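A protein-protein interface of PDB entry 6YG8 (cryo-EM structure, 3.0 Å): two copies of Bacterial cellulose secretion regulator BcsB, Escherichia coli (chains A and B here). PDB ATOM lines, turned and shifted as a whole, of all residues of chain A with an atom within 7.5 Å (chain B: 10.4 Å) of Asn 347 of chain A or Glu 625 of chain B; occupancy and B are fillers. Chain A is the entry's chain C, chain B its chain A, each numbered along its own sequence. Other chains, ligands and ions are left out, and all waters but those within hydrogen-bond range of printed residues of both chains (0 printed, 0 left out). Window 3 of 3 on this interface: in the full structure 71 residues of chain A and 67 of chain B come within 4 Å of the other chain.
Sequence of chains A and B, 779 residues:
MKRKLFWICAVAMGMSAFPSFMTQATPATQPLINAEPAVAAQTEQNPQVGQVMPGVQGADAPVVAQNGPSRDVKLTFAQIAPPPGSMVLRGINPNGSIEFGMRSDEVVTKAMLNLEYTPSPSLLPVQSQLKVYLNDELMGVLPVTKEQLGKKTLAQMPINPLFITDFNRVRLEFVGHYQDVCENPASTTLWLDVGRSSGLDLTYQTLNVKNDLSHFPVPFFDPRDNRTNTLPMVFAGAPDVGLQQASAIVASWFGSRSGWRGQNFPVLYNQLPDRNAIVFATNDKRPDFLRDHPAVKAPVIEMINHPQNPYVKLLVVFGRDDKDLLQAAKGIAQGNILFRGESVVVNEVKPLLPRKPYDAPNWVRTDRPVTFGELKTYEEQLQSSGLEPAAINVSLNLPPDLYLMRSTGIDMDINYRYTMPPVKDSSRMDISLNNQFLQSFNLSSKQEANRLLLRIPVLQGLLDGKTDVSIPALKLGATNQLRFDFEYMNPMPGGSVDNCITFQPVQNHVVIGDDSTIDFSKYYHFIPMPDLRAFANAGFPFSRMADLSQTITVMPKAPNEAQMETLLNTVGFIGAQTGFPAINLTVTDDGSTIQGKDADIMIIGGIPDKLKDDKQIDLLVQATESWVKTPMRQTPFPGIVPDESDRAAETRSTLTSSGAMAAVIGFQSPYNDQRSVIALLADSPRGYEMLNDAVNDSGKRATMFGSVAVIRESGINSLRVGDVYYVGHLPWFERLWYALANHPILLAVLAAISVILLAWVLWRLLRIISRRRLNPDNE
No position is printed for both chains.
Hydrophobic or aromatic side chains of chain B within 4 Å of the printed part of chain A: Val 628, Leu 655 and Met 661.
Along chain B the printed residues that touch a printed residue of chain A span positions 624 to 661.
The side-chain hydroxyl of Thr 656 of chain B is in hydrogen-bond range of the side-chain hydroxyl of Thr 624 of chain B (3.4 Å).
The backbone carbonyl oxygen of Asn 347 of chain A sits at hydrogen-bond distance from the side-chain amide nitrogen of Gln 327 of chain A (3.4 Å).
The backbone carbonyl oxygen (O) of Thr 624 of chain B is in hydrogen-bond range of the guanidinium group (NH2) of Arg 340 of chain A, 2.7 Å away.
The side-chain amide oxygen of Asn 347 of chain A sits close to the backbone carbonyl oxygen of Thr 654 of chain B (2.7 Å).
O of Gly 659 of chain B is in hydrogen-bond range of NE of Arg 340 of chain A, at 3.4 Å.
The backbone carbonyl oxygen (O) of Arg 340 of chain A lies within hydrogen-bond range of the side-chain hydroxyl (OG) of Ser 657 of chain B (2.7 Å).
O of Thr 656 of chain B sits at hydrogen-bond distance from N of Val 345 of chain A (3.2 Å).
The side-chain hydroxyl (OG1) of Thr 654 of chain B lies within hydrogen-bond range of the side-chain carboxylate (OE1) of Glu 348 of chain A (2.6 Å).
Printed residues of chain B within 4 Å of Arg 340 of chain A: Thr 624 (2.7 Å), Ser 626 (3.9 Å), Ser 657 (2.7 Å), Gly 659 (3.4 Å) and Met 661 (3.5 Å).
Of chain B, only Leu 655 comes within 4 Å of Val 346 of chain A.
Of chain A, only Asn 347 comes within 4 Å of Glu 625 of chain B.
Of the printed residues of chain A, Arg 652 of chain B touches Val 349 (3.6 Å).
Of the printed residues of chain A, Thr 654 of chain B touches Asn 347 and Glu 348.
The nearest residue of chain B that does not touch Asn 347 of chain A is Ser 626 of chain B (6.1 Å).
Among the printed residues, merely in contact across the chains: Leu 338 of chain A with Ser 626 of chain B (3.2 Å), Asn 347 of chain A with Thr 656 of chain B (3.3 Å), Val 345 of chain A with Leu 655 of chain B (3.4 Å), Arg 340 of chain A with Met 661 of chain B (3.5 Å), Val 349 of chain A with Arg 652 of chain B (3.6 Å), Asn 347 of chain A with Glu 625 of chain B (3.6 Å), Glu 348 of chain A with Ser 653 of chain B (3.6 Å), Leu 338 of chain A with Leu 655 of chain B (3.7 Å), Leu 338 of chain A with Ser 653 of chain B (3.7 Å), Val 346 of chain A with Leu 655 of chain B (3.7 Å), Leu 338 of chain A with Val 628 of chain B (3.7 Å), Leu 338 of chain A with Trp 627 of chain B (3.8 Å), Leu 338 of chain A with Met 661 of chain B (3.8 Å), Val 344 of chain A with Ser 657 of chain B (3.9 Å), Arg 340 of chain A with Ser 626 of chain B (3.9 Å), Val 344 of chain A with Thr 656 of chain B (3.9 Å), Val 349 of chain A with Ser 653 of chain B (3.9 Å) and Asn 347 of chain A with Leu 655 of chain B (3.96 Å).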
ATOM      1  N   ALA A 298       3.948  22.577   0.220  1.00  0.00           N
ATOM      2  CA  ALA A 298       4.985  21.644   0.626  1.00  0.00           C
ATOM      3  C   ALA A 298       4.336  20.507   1.405  1.00  0.00           C
ATOM      4  O   ALA A 298       3.173  20.629   1.805  1.00  0.00           O
ATOM      5  CB  ALA A 298       6.041  22.364   1.465  1.00  0.00           C
ATOM      6  N   PRO A 299       5.031  19.394   1.646  1.00  0.00           N
ATOM      7  CA  PRO A 299       4.393  18.306   2.394  1.00  0.00           C
ATOM      8  C   PRO A 299       4.186  18.668   3.851  1.00  0.00           C
ATOM      9  O   PRO A 299       5.138  18.676   4.634  1.00  0.00           O
ATOM     10  CB  PRO A 299       5.387  17.145   2.253  1.00  0.00           C
ATOM     11  CG  PRO A 299       6.274  17.515   1.133  1.00  0.00           C
ATOM     12  CD  PRO A 299       6.346  18.998   1.119  1.00  0.00           C
ATOM     13  N   VAL A 300       2.948  18.957   4.228  1.00  0.00           N
ATOM     14  CA  VAL A 300       2.617  19.288   5.599  1.00  0.00           C
ATOM     15  C   VAL A 300       2.074  18.042   6.278  1.00  0.00           C
ATOM     16  O   VAL A 300       1.658  17.078   5.633  1.00  0.00           O
ATOM     17  CB  VAL A 300       1.611  20.455   5.689  1.00  0.00           C
ATOM     18  CG1 VAL A 300       2.087  21.626   4.856  1.00  0.00           C
ATOM     19  CG2 VAL A 300       0.246  20.009   5.235  1.00  0.00           C
ATOM     20  N   GLN A 327       8.045  12.378   0.349  1.00  0.00           N
ATOM     21  CA  GLN A 327       8.891  13.198   1.207  1.00  0.00           C
ATOM     22  C   GLN A 327       8.292  13.333   2.598  1.00  0.00           C
ATOM     23  O   GLN A 327       9.019  13.342   3.597  1.00  0.00           O
ATOM     24  CB  GLN A 327       9.101  14.573   0.578  1.00  0.00           C
ATOM     25  CG  GLN A 327      10.187  15.384   1.246  1.00  0.00           C
ATOM     26  CD  GLN A 327      10.431  16.699   0.548  1.00  0.00           C
ATOM     27  OE1 GLN A 327       9.527  17.266  -0.064  1.00  0.00           O
ATOM     28  NE2 GLN A 327      11.659  17.194   0.629  1.00  0.00           N
ATOM     29  N   ALA A 328       6.967  13.436   2.684  1.00  0.00           N
ATOM     30  CA  ALA A 328       6.321  13.485   3.988  1.00  0.00           C
ATOM     31  C   ALA A 328       6.408  12.142   4.697  1.00  0.00           C
ATOM     32  O   ALA A 328       6.594  12.089   5.916  1.00  0.00           O
ATOM     33  CB  ALA A 328       4.866  13.921   3.836  1.00  0.00           C
ATOM     34  N   LEU A 338      11.736  16.106  15.359  1.00  0.00           N
ATOM     35  CA  LEU A 338      11.512  17.538  15.267  1.00  0.00           C
ATOM     36  C   LEU A 338      10.039  17.883  15.124  1.00  0.00           C
ATOM     37  O   LEU A 338       9.709  19.022  14.785  1.00  0.00           O
ATOM     38  CB  LEU A 338      12.296  18.116  14.092  1.00  0.00           C
ATOM     39  CG  LEU A 338      13.810  17.939  14.156  1.00  0.00           C
ATOM     40  CD1 LEU A 338      14.446  18.480  12.897  1.00  0.00           C
ATOM     41  CD2 LEU A 338      14.360  18.639  15.376  1.00  0.00           C
ATOM     42  N   ARG A 340       6.512  19.092  16.144  1.00  0.00           N
ATOM     43  CA  ARG A 340       6.051  19.998  17.185  1.00  0.00           C
ATOM     44  C   ARG A 340       4.904  20.828  16.638  1.00  0.00           C
ATOM     45  O   ARG A 340       4.834  21.092  15.436  1.00  0.00           O
ATOM     46  CB  ARG A 340       7.181  20.909  17.670  1.00  0.00           C
ATOM     47  CG  ARG A 340       7.856  21.684  16.564  1.00  0.00           C
ATOM     48  CD  ARG A 340       9.178  22.236  17.029  1.00  0.00           C
ATOM     49  NE  ARG A 340       9.699  23.254  16.126  1.00  0.00           N
ATOM     50  CZ  ARG A 340      10.414  22.991  15.040  1.00  0.00           C
ATOM     51  NH1 ARG A 340      10.700  21.738  14.721  1.00  0.00           N
ATOM     52  NH2 ARG A 340      10.848  23.982  14.276  1.00  0.00           N
ATOM     53  N   VAL A 344       3.546  20.338  10.987  1.00  0.00           N
ATOM     54  CA  VAL A 344       4.930  20.485  10.566  1.00  0.00           C
ATOM     55  C   VAL A 344       4.970  20.477   9.043  1.00  0.00           C
ATOM     56  O   VAL A 344       4.012  20.095   8.376  1.00  0.00           O
ATOM     57  CB  VAL A 344       5.839  19.389  11.149  1.00  0.00           C
ATOM     58  CG1 VAL A 344       5.806  19.422  12.661  1.00  0.00           C
ATOM     59  CG2 VAL A 344       5.428  18.034  10.631  1.00  0.00           C
ATOM     60  N   VAL A 345       6.094  20.920   8.494  1.00  0.00           N
ATOM     61  CA  VAL A 345       6.310  20.945   7.054  1.00  0.00           C
ATOM     62  C   VAL A 345       7.637  20.259   6.772  1.00  0.00           C
ATOM     63  O   VAL A 345       8.691  20.742   7.200  1.00  0.00           O
ATOM     64  CB  VAL A 345       6.313  22.375   6.491  1.00  0.00           C
ATOM     65  CG1 VAL A 345       6.648  22.352   5.022  1.00  0.00           C
ATOM     66  CG2 VAL A 345       4.972  23.036   6.721  1.00  0.00           C
ATOM     67  N   VAL A 346       7.587  19.136   6.062  1.00  0.00           N
ATOM     68  CA  VAL A 346       8.785  18.356   5.753  1.00  0.00           C
ATOM     69  C   VAL A 346       9.323  18.896   4.432  1.00  0.00           C
ATOM     70  O   VAL A 346       9.011  18.392   3.355  1.00  0.00           O
ATOM     71  CB  VAL A 346       8.490  16.861   5.694  1.00  0.00           C
ATOM     72  CG1 VAL A 346       9.775  16.078   5.536  1.00  0.00           C
ATOM     73  CG2 VAL A 346       7.746  16.426   6.938  1.00  0.00           C
ATOM     74  N   ASN A 347      10.150  19.935   4.516  1.00  0.00           N
ATOM     75  CA  ASN A 347      10.646  20.596   3.318  1.00  0.00           C
ATOM     76  C   ASN A 347      11.949  20.009   2.797  1.00  0.00           C
ATOM     77  O   ASN A 347      12.373  20.376   1.695  1.00  0.00           O
ATOM     78  CB  ASN A 347      10.832  22.094   3.571  1.00  0.00           C
ATOM     79  CG  ASN A 347      11.507  22.380   4.887  1.00  0.00           C
ATOM     80  OD1 ASN A 347      12.064  21.485   5.515  1.00  0.00           O
ATOM     81  ND2 ASN A 347      11.463  23.633   5.314  1.00  0.00           N
ATOM     82  N   GLU A 348      12.591  19.112   3.541  1.00  0.00           N
ATOM     83  CA  GLU A 348      13.803  18.465   3.051  1.00  0.00           C
ATOM     84  C   GLU A 348      14.109  17.247   3.904  1.00  0.00           C
ATOM     85  O   GLU A 348      14.060  17.319   5.134  1.00  0.00           O
ATOM     86  CB  GLU A 348      14.994  19.425   3.069  1.00  0.00           C
ATOM     87  CG  GLU A 348      16.268  18.829   2.497  1.00  0.00           C
ATOM     88  CD  GLU A 348      17.519  19.420   3.114  1.00  0.00           C
ATOM     89  OE1 GLU A 348      17.466  19.824   4.294  1.00  0.00           O
ATOM     90  OE2 GLU A 348      18.555  19.480   2.419  1.00  0.00           O
ATOM     91  N   VAL A 349      14.426  16.137   3.243  1.00  0.00           N
ATOM     92  CA  VAL A 349      14.938  14.937   3.893  1.00  0.00           C
ATOM     93  C   VAL A 349      16.050  14.393   3.011  1.00  0.00           C
ATOM     94  O   VAL A 349      15.798  13.980   1.874  1.00  0.00           O
ATOM     95  CB  VAL A 349      13.852  13.870   4.110  1.00  0.00           C
ATOM     96  CG1 VAL A 349      14.488  12.527   4.381  1.00  0.00           C
ATOM     97  CG2 VAL A 349      12.952  14.264   5.260  1.00  0.00           C
ATOM     98  N   LYS B 612      28.847  28.311  13.060  1.00  0.00           N
ATOM     99  CA  LYS B 612      27.698  27.558  12.567  1.00  0.00           C
ATOM    100  C   LYS B 612      28.057  26.678  11.378  1.00  0.00           C
ATOM    101  O   LYS B 612      27.431  25.632  11.172  1.00  0.00           O
ATOM    102  CB  LYS B 612      26.573  28.517  12.187  1.00  0.00           C
ATOM    103  CG  LYS B 612      25.220  27.855  12.036  1.00  0.00           C
ATOM    104  CD  LYS B 612      24.247  28.779  11.330  1.00  0.00           C
ATOM    105  CE  LYS B 612      24.228  30.151  11.979  1.00  0.00           C
ATOM    106  NZ  LYS B 612      23.784  30.079  13.397  1.00  0.00           N
ATOM    107  N   LEU B 619      22.482  19.371  14.834  1.00  0.00           N
ATOM    108  CA  LEU B 619      21.146  19.909  15.055  1.00  0.00           C
ATOM    109  C   LEU B 619      21.203  21.424  15.166  1.00  0.00           C
ATOM    110  O   LEU B 619      22.049  21.967  15.880  1.00  0.00           O
ATOM    111  CB  LEU B 619      20.532  19.299  16.316  1.00  0.00           C
ATOM    112  CG  LEU B 619      19.305  19.948  16.956  1.00  0.00           C
ATOM    113  CD1 LEU B 619      18.128  19.952  16.010  1.00  0.00           C
ATOM    114  CD2 LEU B 619      18.950  19.209  18.229  1.00  0.00           C
ATOM    115  N   LEU B 620      20.309  22.115  14.470  1.00  0.00           N
ATOM    116  CA  LEU B 620      20.241  23.564  14.522  1.00  0.00           C
ATOM    117  C   LEU B 620      18.808  23.986  14.796  1.00  0.00           C
ATOM    118  O   LEU B 620      17.859  23.289  14.433  1.00  0.00           O
ATOM    119  CB  LEU B 620      20.738  24.203  13.222  1.00  0.00           C
ATOM    120  CG  LEU B 620      22.212  24.609  13.210  1.00  0.00           C
ATOM    121  CD1 LEU B 620      22.563  25.321  11.916  1.00  0.00           C
ATOM    122  CD2 LEU B 620      22.529  25.484  14.407  1.00  0.00           C
ATOM    123  N   VAL B 621      18.661  25.129  15.453  1.00  0.00           N
ATOM    124  CA  VAL B 621      17.353  25.672  15.808  1.00  0.00           C
ATOM    125  C   VAL B 621      17.322  27.112  15.313  1.00  0.00           C
ATOM    126  O   VAL B 621      17.755  28.040  16.001  1.00  0.00           O
ATOM    127  CB  VAL B 621      17.074  25.590  17.312  1.00  0.00           C
ATOM    128  CG1 VAL B 621      15.682  26.099  17.615  1.00  0.00           C
ATOM    129  CG2 VAL B 621      17.226  24.163  17.800  1.00  0.00           C
ATOM    130  N   GLN B 622      16.798  27.311  14.108  1.00  0.00           N
ATOM    131  CA  GLN B 622      16.531  28.649  13.614  1.00  0.00           C
ATOM    132  C   GLN B 622      15.226  29.165  14.210  1.00  0.00           C
ATOM    133  O   GLN B 622      14.685  28.602  15.165  1.00  0.00           O
ATOM    134  CB  GLN B 622      16.472  28.667  12.087  1.00  0.00           C
ATOM    135  CG  GLN B 622      17.830  28.626  11.406  1.00  0.00           C
ATOM    136  CD  GLN B 622      18.459  27.245  11.428  1.00  0.00           C
ATOM    137  OE1 GLN B 622      19.532  27.050  11.998  1.00  0.00           O
ATOM    138  NE2 GLN B 622      17.797  26.281  10.801  1.00  0.00           N
ATOM    139  N   ALA B 623      14.726  30.268  13.648  1.00  0.00           N
ATOM    140  CA  ALA B 623      13.473  30.834  14.137  1.00  0.00           C
ATOM    141  C   ALA B 623      12.357  29.800  14.113  1.00  0.00           C
ATOM    142  O   ALA B 623      11.812  29.439  15.162  1.00  0.00           O
ATOM    143  CB  ALA B 623      13.089  32.059  13.308  1.00  0.00           C
ATOM    144  N   THR B 624      12.015  29.298  12.932  1.00  0.00           N
ATOM    145  CA  THR B 624      11.084  28.185  12.806  1.00  0.00           C
ATOM    146  C   THR B 624      11.694  26.956  12.156  1.00  0.00           C
ATOM    147  O   THR B 624      11.225  25.847  12.416  1.00  0.00           O
ATOM    148  CB  THR B 624       9.841  28.601  12.004  1.00  0.00           C
ATOM    149  OG1 THR B 624      10.240  29.094  10.719  1.00  0.00           O
ATOM    150  CG2 THR B 624       9.067  29.680  12.741  1.00  0.00           C
ATOM    151  N   GLU B 625      12.723  27.117  11.330  1.00  0.00           N
ATOM    152  CA  GLU B 625      13.342  25.976  10.678  1.00  0.00           C
ATOM    153  C   GLU B 625      14.244  25.228  11.651  1.00  0.00           C
ATOM    154  O   GLU B 625      14.799  25.798  12.594  1.00  0.00           O
ATOM    155  CB  GLU B 625      14.146  26.417   9.457  1.00  0.00           C
ATOM    156  CG  GLU B 625      14.357  25.315   8.435  1.00  0.00           C
ATOM    157  CD  GLU B 625      14.967  25.821   7.146  1.00  0.00           C
ATOM    158  OE1 GLU B 625      15.871  26.680   7.212  1.00  0.00           O
ATOM    159  OE2 GLU B 625      14.542  25.358   6.067  1.00  0.00           O
ATOM    160  N   SER B 626      14.394  23.931  11.401  1.00  0.00           N
ATOM    161  CA  SER B 626      15.193  23.074  12.264  1.00  0.00           C
ATOM    162  C   SER B 626      15.527  21.771  11.554  1.00  0.00           C
ATOM    163  O   SER B 626      14.632  21.097  11.037  1.00  0.00           O
ATOM    164  CB  SER B 626      14.451  22.792  13.570  1.00  0.00           C
ATOM    165  OG  SER B 626      15.198  21.922  14.399  1.00  0.00           O
ATOM    166  N   TRP B 627      16.805  21.409  11.517  1.00  0.00           N
ATOM    167  CA  TRP B 627      17.239  20.165  10.906  1.00  0.00           C
ATOM    168  C   TRP B 627      18.025  19.354  11.925  1.00  0.00           C
ATOM    169  O   TRP B 627      18.555  19.891  12.897  1.00  0.00           O
ATOM    170  CB  TRP B 627      18.091  20.411   9.657  1.00  0.00           C
ATOM    171  CG  TRP B 627      19.300  21.247   9.906  1.00  0.00           C
ATOM    172  CD1 TRP B 627      19.420  22.587   9.708  1.00  0.00           C
ATOM    173  CD2 TRP B 627      20.569  20.797  10.395  1.00  0.00           C
ATOM    174  NE1 TRP B 627      20.682  23.004  10.046  1.00  0.00           N
ATOM    175  CE2 TRP B 627      21.407  21.923  10.471  1.00  0.00           C
ATOM    176  CE3 TRP B 627      21.075  19.553  10.777  1.00  0.00           C
ATOM    177  CZ2 TRP B 627      22.721  21.842  10.913  1.00  0.00           C
ATOM    178  CZ3 TRP B 627      22.377  19.477  11.216  1.00  0.00           C
ATOM    179  CH2 TRP B 627      23.186  20.612  11.279  1.00  0.00           C
ATOM    180  N   VAL B 628      18.106  18.048  11.681  1.00  0.00           N
ATOM    181  CA  VAL B 628      18.766  17.131  12.598  1.00  0.00           C
ATOM    182  C   VAL B 628      19.341  15.975  11.797  1.00  0.00           C
ATOM    183  O   VAL B 628      18.853  15.641  10.715  1.00  0.00           O
ATOM    184  CB  VAL B 628      17.789  16.632  13.692  1.00  0.00           C
ATOM    185  CG1 VAL B 628      16.821  15.610  13.122  1.00  0.00           C
ATOM    186  CG2 VAL B 628      18.547  16.055  14.872  1.00  0.00           C
ATOM    187  N   ARG B 652      19.734  13.348   7.130  1.00  0.00           N
ATOM    188  CA  ARG B 652      19.507  14.690   7.647  1.00  0.00           C
ATOM    189  C   ARG B 652      18.128  15.153   7.205  1.00  0.00           C
ATOM    190  O   ARG B 652      17.823  15.151   6.008  1.00  0.00           O
ATOM    191  CB  ARG B 652      20.577  15.667   7.162  1.00  0.00           C
ATOM    192  CG  ARG B 652      20.230  17.121   7.406  1.00  0.00           C
ATOM    193  CD  ARG B 652      21.386  18.030   7.055  1.00  0.00           C
ATOM    194  NE  ARG B 652      20.935  19.232   6.365  1.00  0.00           N
ATOM    195  CZ  ARG B 652      21.666  20.332   6.229  1.00  0.00           C
ATOM    196  NH1 ARG B 652      21.174  21.381   5.583  1.00  0.00           N
ATOM    197  NH2 ARG B 652      22.886  20.386   6.741  1.00  0.00           N
ATOM    198  N   SER B 653      17.301  15.549   8.167  1.00  0.00           N
ATOM    199  CA  SER B 653      15.904  15.879   7.925  1.00  0.00           C
ATOM    200  C   SER B 653      15.613  17.271   8.463  1.00  0.00           C
ATOM    201  O   SER B 653      15.861  17.549   9.640  1.00  0.00           O
ATOM    202  CB  SER B 653      14.987  14.848   8.580  1.00  0.00           C
ATOM    203  OG  SER B 653      15.137  14.872   9.986  1.00  0.00           O
ATOM    204  N   THR B 654      15.084  18.137   7.605  1.00  0.00           N
ATOM    205  CA  THR B 654      14.744  19.509   7.959  1.00  0.00           C
ATOM    206  C   THR B 654      13.230  19.638   8.034  1.00  0.00           C
ATOM    207  O   THR B 654      12.531  19.301   7.074  1.00  0.00           O
ATOM    208  CB  THR B 654      15.304  20.495   6.934  1.00  0.00           C
ATOM    209  OG1 THR B 654      16.695  20.230   6.723  1.00  0.00           O
ATOM    210  CG2 THR B 654      15.134  21.919   7.422  1.00  0.00           C
ATOM    211  N   LEU B 655      12.729  20.120   9.167  1.00  0.00           N
ATOM    212  CA  LEU B 655      11.312  20.402   9.341  1.00  0.00           C
ATOM    213  C   LEU B 655      11.143  21.802   9.904  1.00  0.00           C
ATOM    214  O   LEU B 655      11.961  22.272  10.697  1.00  0.00           O
ATOM    215  CB  LEU B 655      10.631  19.403  10.278  1.00  0.00           C
ATOM    216  CG  LEU B 655      11.020  17.928  10.237  1.00  0.00           C
ATOM    217  CD1 LEU B 655      10.185  17.193  11.243  1.00  0.00           C
ATOM    218  CD2 LEU B 655      10.809  17.336   8.863  1.00  0.00           C
ATOM    219  N   THR B 656      10.067  22.467   9.492  1.00  0.00           N
ATOM    220  CA  THR B 656       9.756  23.810   9.964  1.00  0.00           C
ATOM    221  C   THR B 656       8.353  23.829  10.551  1.00  0.00           C
ATOM    222  O   THR B 656       7.390  23.442   9.883  1.00  0.00           O
ATOM    223  CB  THR B 656       9.898  24.844   8.842  1.00  0.00           C
ATOM    224  OG1 THR B 656       9.380  26.105   9.281  1.00  0.00           O
ATOM    225  CG2 THR B 656       9.173  24.401   7.583  1.00  0.00           C
ATOM    226  N   SER B 657       8.243  24.260  11.803  1.00  0.00           N
ATOM    227  CA  SER B 657       6.963  24.373  12.482  1.00  0.00           C
ATOM    228  C   SER B 657       6.982  25.611  13.364  1.00  0.00           C
ATOM    229  O   SER B 657       8.030  26.211  13.610  1.00  0.00           O
ATOM    230  CB  SER B 657       6.657  23.124  13.314  1.00  0.00           C
ATOM    231  OG  SER B 657       5.521  23.330  14.134  1.00  0.00           O
ATOM    232  N   SER B 658       5.801  25.995  13.846  1.00  0.00           N
ATOM    233  CA  SER B 658       5.678  27.126  14.752  1.00  0.00           C
ATOM    234  C   SER B 658       5.632  26.708  16.213  1.00  0.00           C
ATOM    235  O   SER B 658       5.614  27.578  17.089  1.00  0.00           O
ATOM    236  CB  SER B 658       4.427  27.945  14.420  1.00  0.00           C
ATOM    237  OG  SER B 658       3.252  27.202  14.686  1.00  0.00           O
ATOM    238  N   GLY B 659       5.608  25.411  16.495  1.00  0.00           N
ATOM    239  CA  GLY B 659       5.676  24.941  17.863  1.00  0.00           C
ATOM    240  C   GLY B 659       6.996  25.301  18.514  1.00  0.00           C
ATOM    241  O   GLY B 659       7.974  25.675  17.871  1.00  0.00           O
ATOM    242  N   ALA B 660       7.016  25.176  19.835  1.00  0.00           N
ATOM    243  CA  ALA B 660       8.176  25.562  20.622  1.00  0.00           C
ATOM    244  C   ALA B 660       9.115  24.381  20.795  1.00  0.00           C
ATOM    245  O   ALA B 660       8.676  23.250  21.017  1.00  0.00           O
ATOM    246  CB  ALA B 660       7.747  26.090  21.988  1.00  0.00           C
ATOM    247  N   MET B 661      10.414  24.653  20.698  1.00  0.00           N
ATOM    248  CA  MET B 661      11.416  23.604  20.814  1.00  0.00           C
ATOM    249  C   MET B 661      12.729  24.214  21.273  1.00  0.00           C
ATOM    250  O   MET B 661      13.152  25.243  20.743  1.00  0.00           O
ATOM    251  CB  MET B 661      11.611  22.882  19.481  1.00  0.00           C
ATOM    252  CG  MET B 661      12.629  21.766  19.525  1.00  0.00           C
ATOM    253  SD  MET B 661      13.204  21.307  17.886  1.00  0.00           S
ATOM    254  CE  MET B 661      13.767  22.893  17.287  1.00  0.00           C
ATOM    255  N   ALA B 662      13.361  23.577  22.250  1.00  0.00           N
ATOM    256  CA  ALA B 662      14.706  23.920  22.672  1.00  0.00           C
ATOM    257  C   ALA B 662      15.613  22.725  22.424  1.00  0.00           C
ATOM    258  O   ALA B 662      15.152  21.590  22.296  1.00  0.00           O
ATOM    259  CB  ALA B 662      14.749  24.319  24.149  1.00  0.00           C
ATOM    260  N   ALA B 663      16.912  22.987  22.354  1.00  0.00           N
ATOM    261  CA  ALA B 663      17.858  21.932  22.036  1.00  0.00           C
ATOM    262  C   ALA B 663      19.165  22.171  22.768  1.00  0.00           C
ATOM    263  O   ALA B 663      19.590  23.311  22.962  1.00  0.00           O
ATOM    264  CB  ALA B 663      18.111  21.844  20.530  1.00  0.00           C
ATOM    265  N   LEU B 681      20.259  25.942  22.853  1.00  0.00           N
ATOM    266  CA  LEU B 681      19.535  26.700  21.845  1.00  0.00           C
ATOM    267  C   LEU B 681      18.052  26.772  22.176  1.00  0.00           C
ATOM    268  O   LEU B 681      17.486  25.868  22.791  1.00  0.00           O
ATOM    269  CB  LEU B 681      19.722  26.075  20.466  1.00  0.00           C
ATOM    270  CG  LEU B 681      21.167  25.805  20.057  1.00  0.00           C
ATOM    271  CD1 LEU B 681      21.220  24.797  18.931  1.00  0.00           C
ATOM    272  CD2 LEU B 681      21.842  27.097  19.653  1.00  0.00           C
ATOM    273  N   ALA B 682      17.427  27.867  21.751  1.00  0.00           N
ATOM    274  CA  ALA B 682      15.994  28.054  21.926  1.00  0.00           C
ATOM    275  C   ALA B 682      15.523  29.077  20.907  1.00  0.00           C
ATOM    276  O   ALA B 682      16.139  30.135  20.761  1.00  0.00           O
ATOM    277  CB  ALA B 682      15.663  28.513  23.344  1.00  0.00           C
ATOM    278  N   ASP B 683      14.434  28.760  20.209  1.00  0.00           N
ATOM    279  CA  ASP B 683      13.994  29.599  19.100  1.00  0.00           C
ATOM    280  C   ASP B 683      13.117  30.755  19.564  1.00  0.00           C
ATOM    281  O   ASP B 683      13.254  31.876  19.065  1.00  0.00           O
ATOM    282  CB  ASP B 683      13.245  28.751  18.073  1.00  0.00           C
ATOM    283  CG  ASP B 683      12.113  27.957  18.690  1.00  0.00           C
ATOM    284  OD1 ASP B 683      12.146  27.726  19.916  1.00  0.00           O
ATOM    285  OD2 ASP B 683      11.190  27.564  17.948  1.00  0.00           O
ATOM    286  N   SER B 684      12.222  30.506  20.507  1.00  0.00           N
ATOM    287  CA  SER B 684      11.175  31.441  20.888  1.00  0.00           C
ATOM    288  C   SER B 684      11.134  31.604  22.395  1.00  0.00           C
ATOM    289  O   SER B 684      11.721  30.808  23.134  1.00  0.00           O
ATOM    290  CB  SER B 684       9.817  30.943  20.369  1.00  0.00           C
ATOM    291  OG  SER B 684       9.454  29.723  20.988  1.00  0.00           O
